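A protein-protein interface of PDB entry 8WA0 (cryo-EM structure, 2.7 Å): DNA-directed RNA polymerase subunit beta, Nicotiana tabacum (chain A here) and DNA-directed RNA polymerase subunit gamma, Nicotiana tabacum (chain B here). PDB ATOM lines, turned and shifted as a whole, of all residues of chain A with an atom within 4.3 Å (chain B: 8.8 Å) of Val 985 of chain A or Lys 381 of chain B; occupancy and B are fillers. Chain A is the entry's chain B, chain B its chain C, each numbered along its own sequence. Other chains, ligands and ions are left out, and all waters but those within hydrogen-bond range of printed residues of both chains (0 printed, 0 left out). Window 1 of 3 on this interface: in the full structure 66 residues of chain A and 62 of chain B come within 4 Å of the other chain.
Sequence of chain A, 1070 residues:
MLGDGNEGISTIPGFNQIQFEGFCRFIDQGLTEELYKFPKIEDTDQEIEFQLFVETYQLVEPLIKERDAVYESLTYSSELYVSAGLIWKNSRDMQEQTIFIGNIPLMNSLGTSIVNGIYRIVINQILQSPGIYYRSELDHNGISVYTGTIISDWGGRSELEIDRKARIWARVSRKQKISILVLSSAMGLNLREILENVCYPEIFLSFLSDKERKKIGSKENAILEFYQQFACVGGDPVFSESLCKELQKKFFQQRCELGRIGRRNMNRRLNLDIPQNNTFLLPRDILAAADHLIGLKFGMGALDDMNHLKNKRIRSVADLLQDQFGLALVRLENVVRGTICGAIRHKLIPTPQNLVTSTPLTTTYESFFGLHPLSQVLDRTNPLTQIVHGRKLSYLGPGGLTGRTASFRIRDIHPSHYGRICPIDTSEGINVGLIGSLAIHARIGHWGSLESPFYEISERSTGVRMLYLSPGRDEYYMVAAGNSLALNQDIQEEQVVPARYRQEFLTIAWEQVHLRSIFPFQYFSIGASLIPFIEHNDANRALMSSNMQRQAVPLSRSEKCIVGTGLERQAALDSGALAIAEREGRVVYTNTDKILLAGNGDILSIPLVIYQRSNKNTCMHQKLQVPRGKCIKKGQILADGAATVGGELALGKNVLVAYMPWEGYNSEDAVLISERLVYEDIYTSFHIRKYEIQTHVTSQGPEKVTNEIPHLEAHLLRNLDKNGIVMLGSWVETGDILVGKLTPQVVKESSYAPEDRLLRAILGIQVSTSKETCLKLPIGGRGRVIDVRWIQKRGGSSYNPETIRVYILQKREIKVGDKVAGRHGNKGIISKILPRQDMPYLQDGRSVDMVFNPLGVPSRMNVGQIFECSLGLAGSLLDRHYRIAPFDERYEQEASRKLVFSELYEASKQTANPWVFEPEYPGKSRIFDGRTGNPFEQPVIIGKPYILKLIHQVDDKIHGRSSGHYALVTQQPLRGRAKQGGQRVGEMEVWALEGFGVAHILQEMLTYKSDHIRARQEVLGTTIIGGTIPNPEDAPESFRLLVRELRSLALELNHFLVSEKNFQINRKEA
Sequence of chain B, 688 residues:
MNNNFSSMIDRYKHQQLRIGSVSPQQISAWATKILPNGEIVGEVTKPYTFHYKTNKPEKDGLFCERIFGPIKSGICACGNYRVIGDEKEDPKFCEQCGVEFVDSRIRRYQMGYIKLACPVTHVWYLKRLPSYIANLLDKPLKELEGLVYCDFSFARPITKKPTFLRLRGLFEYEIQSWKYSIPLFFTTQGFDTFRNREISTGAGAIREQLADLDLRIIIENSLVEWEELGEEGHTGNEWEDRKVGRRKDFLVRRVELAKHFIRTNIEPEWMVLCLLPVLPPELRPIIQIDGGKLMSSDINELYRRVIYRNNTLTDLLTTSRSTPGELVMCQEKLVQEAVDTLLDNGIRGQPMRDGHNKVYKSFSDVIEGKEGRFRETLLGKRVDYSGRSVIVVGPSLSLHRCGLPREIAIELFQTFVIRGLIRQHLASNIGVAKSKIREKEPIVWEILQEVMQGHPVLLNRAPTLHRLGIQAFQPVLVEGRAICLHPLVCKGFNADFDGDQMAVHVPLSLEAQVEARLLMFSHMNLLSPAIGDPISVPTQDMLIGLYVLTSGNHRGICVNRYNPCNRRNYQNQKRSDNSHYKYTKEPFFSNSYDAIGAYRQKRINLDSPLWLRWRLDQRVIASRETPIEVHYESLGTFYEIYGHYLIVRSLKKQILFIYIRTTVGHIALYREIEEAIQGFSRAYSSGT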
ATOM      1  N   GLN A 972      25.415  21.652  -2.705  1.00  0.00           N
ATOM      2  CA  GLN A 972      24.508  20.677  -2.150  1.00  0.00           C
ATOM      3  C   GLN A 972      23.880  19.839  -3.272  1.00  0.00           C
ATOM      4  O   GLN A 972      24.049  20.172  -4.437  1.00  0.00           O
ATOM      5  CB  GLN A 972      23.428  21.338  -1.300  1.00  0.00           C
ATOM      6  CG  GLN A 972      23.935  21.913   0.007  1.00  0.00           C
ATOM      7  CD  GLN A 972      22.833  22.553   0.816  1.00  0.00           C
ATOM      8  OE1 GLN A 972      21.658  22.433   0.484  1.00  0.00           O
ATOM      9  NE2 GLN A 972      23.207  23.235   1.887  1.00  0.00           N
ATOM     10  N   GLN A 983      16.593  14.474  -1.535  1.00  0.00           N
ATOM     11  CA  GLN A 983      15.407  14.858  -0.858  1.00  0.00           C
ATOM     12  C   GLN A 983      15.773  15.744   0.329  1.00  0.00           C
ATOM     13  O   GLN A 983      16.865  15.635   0.842  1.00  0.00           O
ATOM     14  CB  GLN A 983      14.616  13.610  -0.473  1.00  0.00           C
ATOM     15  CG  GLN A 983      14.429  12.561  -1.548  1.00  0.00           C
ATOM     16  CD  GLN A 983      13.346  12.900  -2.534  1.00  0.00           C
ATOM     17  OE1 GLN A 983      12.593  13.849  -2.346  1.00  0.00           O
ATOM     18  NE2 GLN A 983      13.254  12.119  -3.594  1.00  0.00           N
ATOM     19  N   ARG A 984      14.896  16.630   0.761  1.00  0.00           N
ATOM     20  CA  ARG A 984      15.171  17.557   1.847  1.00  0.00           C
ATOM     21  C   ARG A 984      14.963  17.124   3.268  1.00  0.00           C
ATOM     22  O   ARG A 984      13.956  16.519   3.582  1.00  0.00           O
ATOM     23  CB  ARG A 984      14.328  18.800   1.660  1.00  0.00           C
ATOM     24  CG  ARG A 984      14.688  19.937   2.592  1.00  0.00           C
ATOM     25  CD  ARG A 984      14.197  21.273   2.076  1.00  0.00           C
ATOM     26  NE  ARG A 984      14.562  22.358   2.980  1.00  0.00           N
ATOM     27  CZ  ARG A 984      15.710  23.023   2.930  1.00  0.00           C
ATOM     28  NH1 ARG A 984      16.618  22.723   2.014  1.00  0.00           N
ATOM     29  NH2 ARG A 984      15.950  23.994   3.799  1.00  0.00           N
ATOM     30  N   VAL A 985      15.905  17.395   4.147  1.00  0.00           N
ATOM     31  CA  VAL A 985      15.696  17.163   5.545  1.00  0.00           C
ATOM     32  C   VAL A 985      15.602  18.592   5.974  1.00  0.00           C
ATOM     33  O   VAL A 985      16.564  19.312   5.865  1.00  0.00           O
ATOM     34  CB  VAL A 985      16.877  16.460   6.192  1.00  0.00           C
ATOM     35  CG1 VAL A 985      16.708  16.386   7.696  1.00  0.00           C
ATOM     36  CG2 VAL A 985      17.053  15.079   5.594  1.00  0.00           C
ATOM     37  N   GLY A 986      14.470  19.028   6.459  1.00  0.00           N
ATOM     38  CA  GLY A 986      14.265  20.396   6.779  1.00  0.00           C
ATOM     39  C   GLY A 986      14.093  20.631   8.211  1.00  0.00           C
ATOM     40  O   GLY A 986      14.451  19.789   9.020  1.00  0.00           O
ATOM     41  N   GLU A 989      11.924  18.165  10.262  1.00  0.00           N
ATOM     42  CA  GLU A 989      12.526  16.854  10.376  1.00  0.00           C
ATOM     43  C   GLU A 989      13.650  16.812  11.389  1.00  0.00           C
ATOM     44  O   GLU A 989      13.771  15.846  12.117  1.00  0.00           O
ATOM     45  CB  GLU A 989      12.992  16.412   9.009  1.00  0.00           C
ATOM     46  CG  GLU A 989      13.438  14.971   8.929  1.00  0.00           C
ATOM     47  CD  GLU A 989      13.423  14.445   7.512  1.00  0.00           C
ATOM     48  OE1 GLU A 989      12.932  15.166   6.620  1.00  0.00           O
ATOM     49  OE2 GLU A 989      13.896  13.310   7.293  1.00  0.00           O
ATOM     50  N   MET A1005      23.509  13.382   8.036  1.00  0.00           N
ATOM     51  CA  MET A1005      22.707  14.037   7.028  1.00  0.00           C
ATOM     52  C   MET A1005      23.242  15.412   6.731  1.00  0.00           C
ATOM     53  O   MET A1005      23.206  15.862   5.601  1.00  0.00           O
ATOM     54  CB  MET A1005      21.252  14.097   7.455  1.00  0.00           C
ATOM     55  CG  MET A1005      20.612  12.727   7.509  1.00  0.00           C
ATOM     56  SD  MET A1005      18.863  12.806   7.887  1.00  0.00           S
ATOM     57  CE  MET A1005      18.389  11.102   7.632  1.00  0.00           C
ATOM     58  N   LEU A1006      23.724  16.099   7.744  1.00  0.00           N
ATOM     59  CA  LEU A1006      24.256  17.431   7.550  1.00  0.00           C
ATOM     60  C   LEU A1006      25.672  17.495   6.987  1.00  0.00           C
ATOM     61  O   LEU A1006      26.076  18.547   6.519  1.00  0.00           O
ATOM     62  CB  LEU A1006      24.224  18.186   8.869  1.00  0.00           C
ATOM     63  CG  LEU A1006      22.900  18.217   9.624  1.00  0.00           C
ATOM     64  CD1 LEU A1006      23.113  18.805  11.008  1.00  0.00           C
ATOM     65  CD2 LEU A1006      21.849  19.001   8.857  1.00  0.00           C
ATOM     66  N   SER A1010      25.460  15.560   2.509  1.00  0.00           N
ATOM     67  CA  SER A1010      25.296  16.838   1.849  1.00  0.00           C
ATOM     68  C   SER A1010      26.459  17.735   2.139  1.00  0.00           C
ATOM     69  O   SER A1010      26.788  17.915   3.298  1.00  0.00           O
ATOM     70  CB  SER A1010      24.076  17.523   2.398  1.00  0.00           C
ATOM     71  OG  SER A1010      23.904  18.787   1.795  1.00  0.00           O
ATOM     72  N   SER A1038      28.417  24.980   3.986  1.00  0.00           N
ATOM     73  CA  SER A1038      27.395  25.910   4.417  1.00  0.00           C
ATOM     74  C   SER A1038      27.898  26.902   5.445  1.00  0.00           C
ATOM     75  O   SER A1038      27.557  28.074   5.391  1.00  0.00           O
ATOM     76  CB  SER A1038      26.217  25.142   4.987  1.00  0.00           C
ATOM     77  OG  SER A1038      25.573  24.390   3.978  1.00  0.00           O
ATOM     78  N   ARG B 373      20.253  32.863   4.164  1.00  0.00           N
ATOM     79  CA  ARG B 373      21.199  31.782   4.347  1.00  0.00           C
ATOM     80  C   ARG B 373      20.878  30.904   5.532  1.00  0.00           C
ATOM     81  O   ARG B 373      20.799  29.688   5.402  1.00  0.00           O
ATOM     82  CB  ARG B 373      22.616  32.346   4.473  1.00  0.00           C
ATOM     83  CG  ARG B 373      23.718  31.300   4.502  1.00  0.00           C
ATOM     84  CD  ARG B 373      24.385  31.106   3.148  1.00  0.00           C
ATOM     85  NE  ARG B 373      23.484  30.574   2.127  1.00  0.00           N
ATOM     86  CZ  ARG B 373      22.978  31.289   1.125  1.00  0.00           C
ATOM     87  NH1 ARG B 373      23.290  32.569   0.997  1.00  0.00           N
ATOM     88  NH2 ARG B 373      22.167  30.720   0.247  1.00  0.00           N
ATOM     89  N   PHE B 374      20.666  31.500   6.692  1.00  0.00           N
ATOM     90  CA  PHE B 374      20.494  30.661   7.858  1.00  0.00           C
ATOM     91  C   PHE B 374      19.290  29.731   7.827  1.00  0.00           C
ATOM     92  O   PHE B 374      19.439  28.543   8.079  1.00  0.00           O
ATOM     93  CB  PHE B 374      20.425  31.534   9.105  1.00  0.00           C
ATOM     94  N   ARG B 375      18.107  30.225   7.502  1.00  0.00           N
ATOM     95  CA  ARG B 375      16.992  29.294   7.435  1.00  0.00           C
ATOM     96  C   ARG B 375      17.022  28.334   6.265  1.00  0.00           C
ATOM     97  O   ARG B 375      16.800  27.140   6.433  1.00  0.00           O
ATOM     98  CB  ARG B 375      15.660  30.025   7.508  1.00  0.00           C
ATOM     99  CG  ARG B 375      15.268  30.443   8.916  1.00  0.00           C
ATOM    100  CD  ARG B 375      13.881  31.064   8.939  1.00  0.00           C
ATOM    101  NE  ARG B 375      12.915  30.258   8.198  1.00  0.00           N
ATOM    102  CZ  ARG B 375      12.153  29.313   8.736  1.00  0.00           C
ATOM    103  NH1 ARG B 375      12.232  29.048  10.032  1.00  0.00           N
ATOM    104  NH2 ARG B 375      11.308  28.634   7.975  1.00  0.00           N
ATOM    105  N   GLU B 376      17.300  28.854   5.078  1.00  0.00           N
ATOM    106  CA  GLU B 376      17.285  28.012   3.892  1.00  0.00           C
ATOM    107  C   GLU B 376      18.364  26.970   3.816  1.00  0.00           C
ATOM    108  O   GLU B 376      18.100  25.836   3.439  1.00  0.00           O
ATOM    109  CB  GLU B 376      17.348  28.862   2.631  1.00  0.00           C
ATOM    110  N   THR B 377      19.592  27.340   4.141  1.00  0.00           N
ATOM    111  CA  THR B 377      20.674  26.384   3.969  1.00  0.00           C
ATOM    112  C   THR B 377      21.184  25.769   5.248  1.00  0.00           C
ATOM    113  O   THR B 377      21.417  24.570   5.307  1.00  0.00           O
ATOM    114  CB  THR B 377      21.851  26.983   3.173  1.00  0.00           C
ATOM    115  OG1 THR B 377      22.339  28.153   3.834  1.00  0.00           O
ATOM    116  CG2 THR B 377      21.413  27.355   1.770  1.00  0.00           C
ATOM    117  N   LEU B 378      21.382  26.582   6.270  1.00  0.00           N
ATOM    118  CA  LEU B 378      21.959  26.071   7.500  1.00  0.00           C
ATOM    119  C   LEU B 378      21.120  25.062   8.272  1.00  0.00           C
ATOM    120  O   LEU B 378      21.657  24.083   8.774  1.00  0.00           O
ATOM    121  CB  LEU B 378      22.382  27.229   8.392  1.00  0.00           C
ATOM    122  N   LEU B 379      19.813  25.274   8.362  1.00  0.00           N
ATOM    123  CA  LEU B 379      18.964  24.396   9.176  1.00  0.00           C
ATOM    124  C   LEU B 379      18.554  23.121   8.477  1.00  0.00           C
ATOM    125  O   LEU B 379      18.323  22.113   9.128  1.00  0.00           O
ATOM    126  CB  LEU B 379      17.729  25.157   9.629  1.00  0.00           C
ATOM    127  CG  LEU B 379      18.022  26.463  10.369  1.00  0.00           C
ATOM    128  CD1 LEU B 379      16.728  27.144  10.778  1.00  0.00           C
ATOM    129  CD2 LEU B 379      18.915  26.224  11.577  1.00  0.00           C
ATOM    130  N   GLY B 380      18.441  23.155   7.163  1.00  0.00           N
ATOM    131  CA  GLY B 380      18.113  21.983   6.384  1.00  0.00           C
ATOM    132  C   GLY B 380      18.715  21.947   5.011  1.00  0.00           C
ATOM    133  O   GLY B 380      18.879  22.978   4.377  1.00  0.00           O
ATOM    134  N   LYS B 381      19.029  20.754   4.537  1.00  0.00           N
ATOM    135  CA  LYS B 381      19.679  20.630   3.254  1.00  0.00           C
ATOM    136  C   LYS B 381      19.287  19.377   2.507  1.00  0.00           C
ATOM    137  O   LYS B 381      18.798  18.432   3.100  1.00  0.00           O
ATOM    138  CB  LYS B 381      21.182  20.662   3.474  1.00  0.00           C
ATOM    139  CG  LYS B 381      21.645  19.859   4.673  1.00  0.00           C
ATOM    140  CD  LYS B 381      23.112  20.116   4.946  1.00  0.00           C
ATOM    141  CE  LYS B 381      23.377  21.596   5.148  1.00  0.00           C
ATOM    142  NZ  LYS B 381      24.821  21.845   5.392  1.00  0.00           N
ATOM    143  N   ARG B 382      19.492  19.366   1.201  1.00  0.00           N
ATOM    144  CA  ARG B 382      19.199  18.186   0.415  1.00  0.00           C
ATOM    145  C   ARG B 382      20.248  17.145   0.705  1.00  0.00           C
ATOM    146  O   ARG B 382      21.365  17.501   1.004  1.00  0.00           O
ATOM    147  CB  ARG B 382      19.194  18.523  -1.066  1.00  0.00           C
ATOM    148  CG  ARG B 382      18.447  19.793  -1.424  1.00  0.00           C
ATOM    149  CD  ARG B 382      16.951  19.591  -1.325  1.00  0.00           C
ATOM    150  NE  ARG B 382      16.425  18.821  -2.443  1.00  0.00           N
ATOM    151  CZ  ARG B 382      15.166  18.408  -2.522  1.00  0.00           C
ATOM    152  NH1 ARG B 382      14.319  18.687  -1.552  1.00  0.00           N
ATOM    153  NH2 ARG B 382      14.744  17.720  -3.571  1.00  0.00           N
ATOM    154  N   VAL B 383      19.914  15.867   0.610  1.00  0.00           N
ATOM    155  CA  VAL B 383      20.819  14.788   0.937  1.00  0.00           C
ATOM    156  C   VAL B 383      20.876  13.705  -0.116  1.00  0.00           C
ATOM    157  O   VAL B 383      20.015  13.641  -0.963  1.00  0.00           O
ATOM    158  CB  VAL B 383      20.420  14.136   2.259  1.00  0.00           C
ATOM    159  CG1 VAL B 383      20.537  15.104   3.418  1.00  0.00           C
ATOM    160  CG2 VAL B 383      19.032  13.534   2.191  1.00  0.00           C
ATOM    161  N   ASP B 384      21.902  12.861  -0.078  1.00  0.00           N
ATOM    162  CA  ASP B 384      22.024  11.759  -1.026  1.00  0.00           C
ATOM    163  C   ASP B 384      21.457  10.533  -0.401  1.00  0.00           C
ATOM    164  O   ASP B 384      20.976  10.583   0.720  1.00  0.00           O
ATOM    165  CB  ASP B 384      23.474  11.449  -1.336  1.00  0.00           C
ATOM    166  CG  ASP B 384      24.158  12.547  -2.086  1.00  0.00           C
ATOM    167  OD1 ASP B 384      23.478  13.513  -2.461  1.00  0.00           O
ATOM    168  OD2 ASP B 384      25.379  12.441  -2.303  1.00  0.00           O
ATOM    169  N   SER B 386      18.731   8.960  -0.988  1.00  0.00           N
ATOM    170  CA  SER B 386      17.345   9.194  -0.650  1.00  0.00           C
ATOM    171  C   SER B 386      16.416   8.884  -1.825  1.00  0.00           C
ATOM    172  O   SER B 386      16.850   8.918  -2.966  1.00  0.00           O
ATOM    173  CB  SER B 386      17.200  10.642  -0.245  1.00  0.00           C
ATOM    174  N   LEU B 458      14.901   4.474   6.769  1.00  0.00           N
ATOM    175  CA  LEU B 458      14.061   5.448   7.445  1.00  0.00           C
ATOM    176  C   LEU B 458      13.019   6.029   6.525  1.00  0.00           C
ATOM    177  O   LEU B 458      13.328   6.351   5.400  1.00  0.00           O
ATOM    178  CB  LEU B 458      14.913   6.576   8.003  1.00  0.00           C
ATOM    179  CG  LEU B 458      15.321   6.614   9.471  1.00  0.00           C
ATOM    180  CD1 LEU B 458      16.240   5.460   9.815  1.00  0.00           C
ATOM    181  CD2 LEU B 458      16.021   7.930   9.740  1.00  0.00           C
ATOM    182  N   ASN B 460       9.777   8.947   5.961  1.00  0.00           N
ATOM    183  CA  ASN B 460       9.063  10.125   6.475  1.00  0.00           C
ATOM    184  C   ASN B 460       7.987  10.688   5.583  1.00  0.00           C
ATOM    185  O   ASN B 460       8.103  10.640   4.374  1.00  0.00           O
ATOM    186  CB  ASN B 460      10.009  11.253   6.870  1.00  0.00           C
ATOM    187  CG  ASN B 460      10.631  11.945   5.690  1.00  0.00           C
ATOM    188  OD1 ASN B 460      11.297  11.321   4.874  1.00  0.00           O
ATOM    189  ND2 ASN B 460      10.439  13.252   5.610  1.00  0.00           N
ATOM    190  N   ILE B 470       8.838  10.304  11.543  1.00  0.00           N
ATOM    191  CA  ILE B 470       9.919   9.479  11.016  1.00  0.00           C
ATOM    192  C   ILE B 470      10.054   8.203  11.824  1.00  0.00           C
ATOM    193  O   ILE B 470      10.206   8.275  13.025  1.00  0.00           O
ATOM    194  CB  ILE B 470      11.258  10.202  11.098  1.00  0.00           C
ATOM    195  CG1 ILE B 470      11.087  11.680  10.800  1.00  0.00           C
ATOM    196  CG2 ILE B 470      12.262   9.581  10.145  1.00  0.00           C
ATOM    197  CD1 ILE B 470      12.340  12.463  11.070  1.00  0.00           C
ATOM    198  N   ALA B 503       9.145   9.492   1.713  1.00  0.00           N
ATOM    199  CA  ALA B 503      10.552   9.522   1.363  1.00  0.00           C
ATOM    200  C   ALA B 503      11.409   8.537   2.134  1.00  0.00           C
ATOM    201  O   ALA B 503      11.152   8.293   3.294  1.00  0.00           O
ATOM    202  CB  ALA B 503      11.084  10.910   1.546  1.00  0.00           C
ATOM    203  N   VAL B 504      12.431   7.970   1.503  1.00  0.00           N
ATOM    204  CA  VAL B 504      13.283   6.965   2.135  1.00  0.00           C
ATOM    205  C   VAL B 504      14.730   7.395   2.276  1.00  0.00           C
ATOM    206  O   VAL B 504      15.285   7.925   1.342  1.00  0.00           O
ATOM    207  CB  VAL B 504      13.319   5.689   1.292  1.00  0.00           C
ATOM    208  CG1 VAL B 504      13.546   4.475   2.171  1.00  0.00           C
ATOM    209  CG2 VAL B 504      12.050   5.536   0.478  1.00  0.00           C
ATOM    210  N   HIS B 505      15.350   7.175   3.428  1.00  0.00           N
ATOM    211  CA  HIS B 505      16.758   7.485   3.623  1.00  0.00           C
ATOM    212  C   HIS B 505      17.476   6.265   4.175  1.00  0.00           C
ATOM    213  O   HIS B 505      16.890   5.529   4.943  1.00  0.00           O
ATOM    214  CB  HIS B 505      16.903   8.602   4.626  1.00  0.00           C
ATOM    215  CG  HIS B 505      16.244   9.883   4.221  1.00  0.00           C
ATOM    216  ND1 HIS B 505      15.056  10.314   4.769  1.00  0.00           N
ATOM    217  CD2 HIS B 505      16.620  10.838   3.340  1.00  0.00           C
ATOM    218  CE1 HIS B 505      14.723  11.475   4.234  1.00  0.00           C
ATOM    219  NE2 HIS B 505      15.655  11.814   3.363  1.00  0.00           N
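Val 985 of chain A touches just these residues of chain B: Gly 380 and Lys 381. Of the printed residues of chain A, Lys 381 of chain B touches Gln 972 (3.5 Å), Arg 984 (3.9 Å), Val 985 (3.1 Å), Leu 1006 (3.7 Å), Ser 1010 (3.5 Å) and Ser 1038 (3.0 Å). Gly 986 of chain A touches none of the printed residues of chain B. Of the printed residues of chain B, Met 1005 of chain A touches Val 383. Printed residues of chain A within 4 Å of Val 383 of chain B: Gln 983 and Met 1005. The nearest residue of chain B that does not touch Val 985 of chain A is Val 383 of chain B (4.1 Å). The nearest residue of chain A that does not touch Lys 381 of chain B is Gln 983 of chain A (4.1 Å).
The backbone carbonyl oxygen (O) of His 505 of chain B sits at hydrogen-bond distance from the backbone NH (N) of Leu 458 of chain B (2.9 Å). The backbone NH (N) of Asn 460 of chain B lies within hydrogen-bond range of the backbone carbonyl oxygen (O) of Ala 503 of chain B. The side-chain amide nitrogen of Gln 972 of chain A sits at hydrogen-bond distance from the side-chain hydroxyl of Ser 1038 of chain A, 3.4 Å away.
The side-chain carboxylate (OE1) of Glu 989 of chain A is in hydrogen-bond range of the side-chain amide nitrogen (ND2) of Asn 460 of chain B, at 3.3 Å. The backbone carbonyl oxygen (O) of Gln 983 of chain A is in hydrogen-bond range of the backbone NH (N) of Val 383 of chain B, at 3.1 Å. OG of Ser 1038 of chain A sits at hydrogen-bond distance from NZ of Lys 381 of chain B (3.0 Å). The backbone carbonyl oxygen (O) of Arg 382 of chain B sits at hydrogen-bond distance from the side-chain hydroxyl (OG) of Ser 1010 of chain A (3.0 Å). The guanidinium group of Arg 984 of chain A lies within hydrogen-bond range of the backbone carbonyl oxygen of Gly 380 of chain B (3.2 Å). The guanidinium group of Arg 984 of chain A sits at hydrogen-bond distance from the backbone carbonyl oxygen of Glu 376 of chain B, at 2.9 Å. The backbone NH (N) of Arg 984 of chain A lies close to the guanidinium group (NH1) of Arg 382 of chain B. The backbone carbonyl oxygen (O) of Val 985 of chain A sits at hydrogen-bond distance from the backbone NH (N) of Lys 381 of chain B (3.1 Å).
Along chain A the printed residues that touch a printed residue of chain B span positions 972 to 1038. Among the printed residues, no Asp or Glu carboxylate lies within 4 Å of a Lys or Arg side-chain nitrogen of the other chain.
Among the printed residues, merely in contact across the chains: Gln 972 of chain A with Lys 381 of chain B, Gln 972 of chain A with Arg 382 of chain B, Gln 983 of chain A with Arg 382 of chain B, Gln 983 of chain A with Ser 386 of chain B, Arg 984 of chain A with Lys 381 of chain B, Val 985 of chain A with Gly 380 of chain B, Glu 989 of chain A with Ile 470 of chain B, Glu 989 of chain A with His 505 of chain B, Met 1005 of chain A with Val 383 of chain B, Leu 1006 of chain A with Lys 381 of chain B and Ser 1010 of chain A with Lys 381 of chain B.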
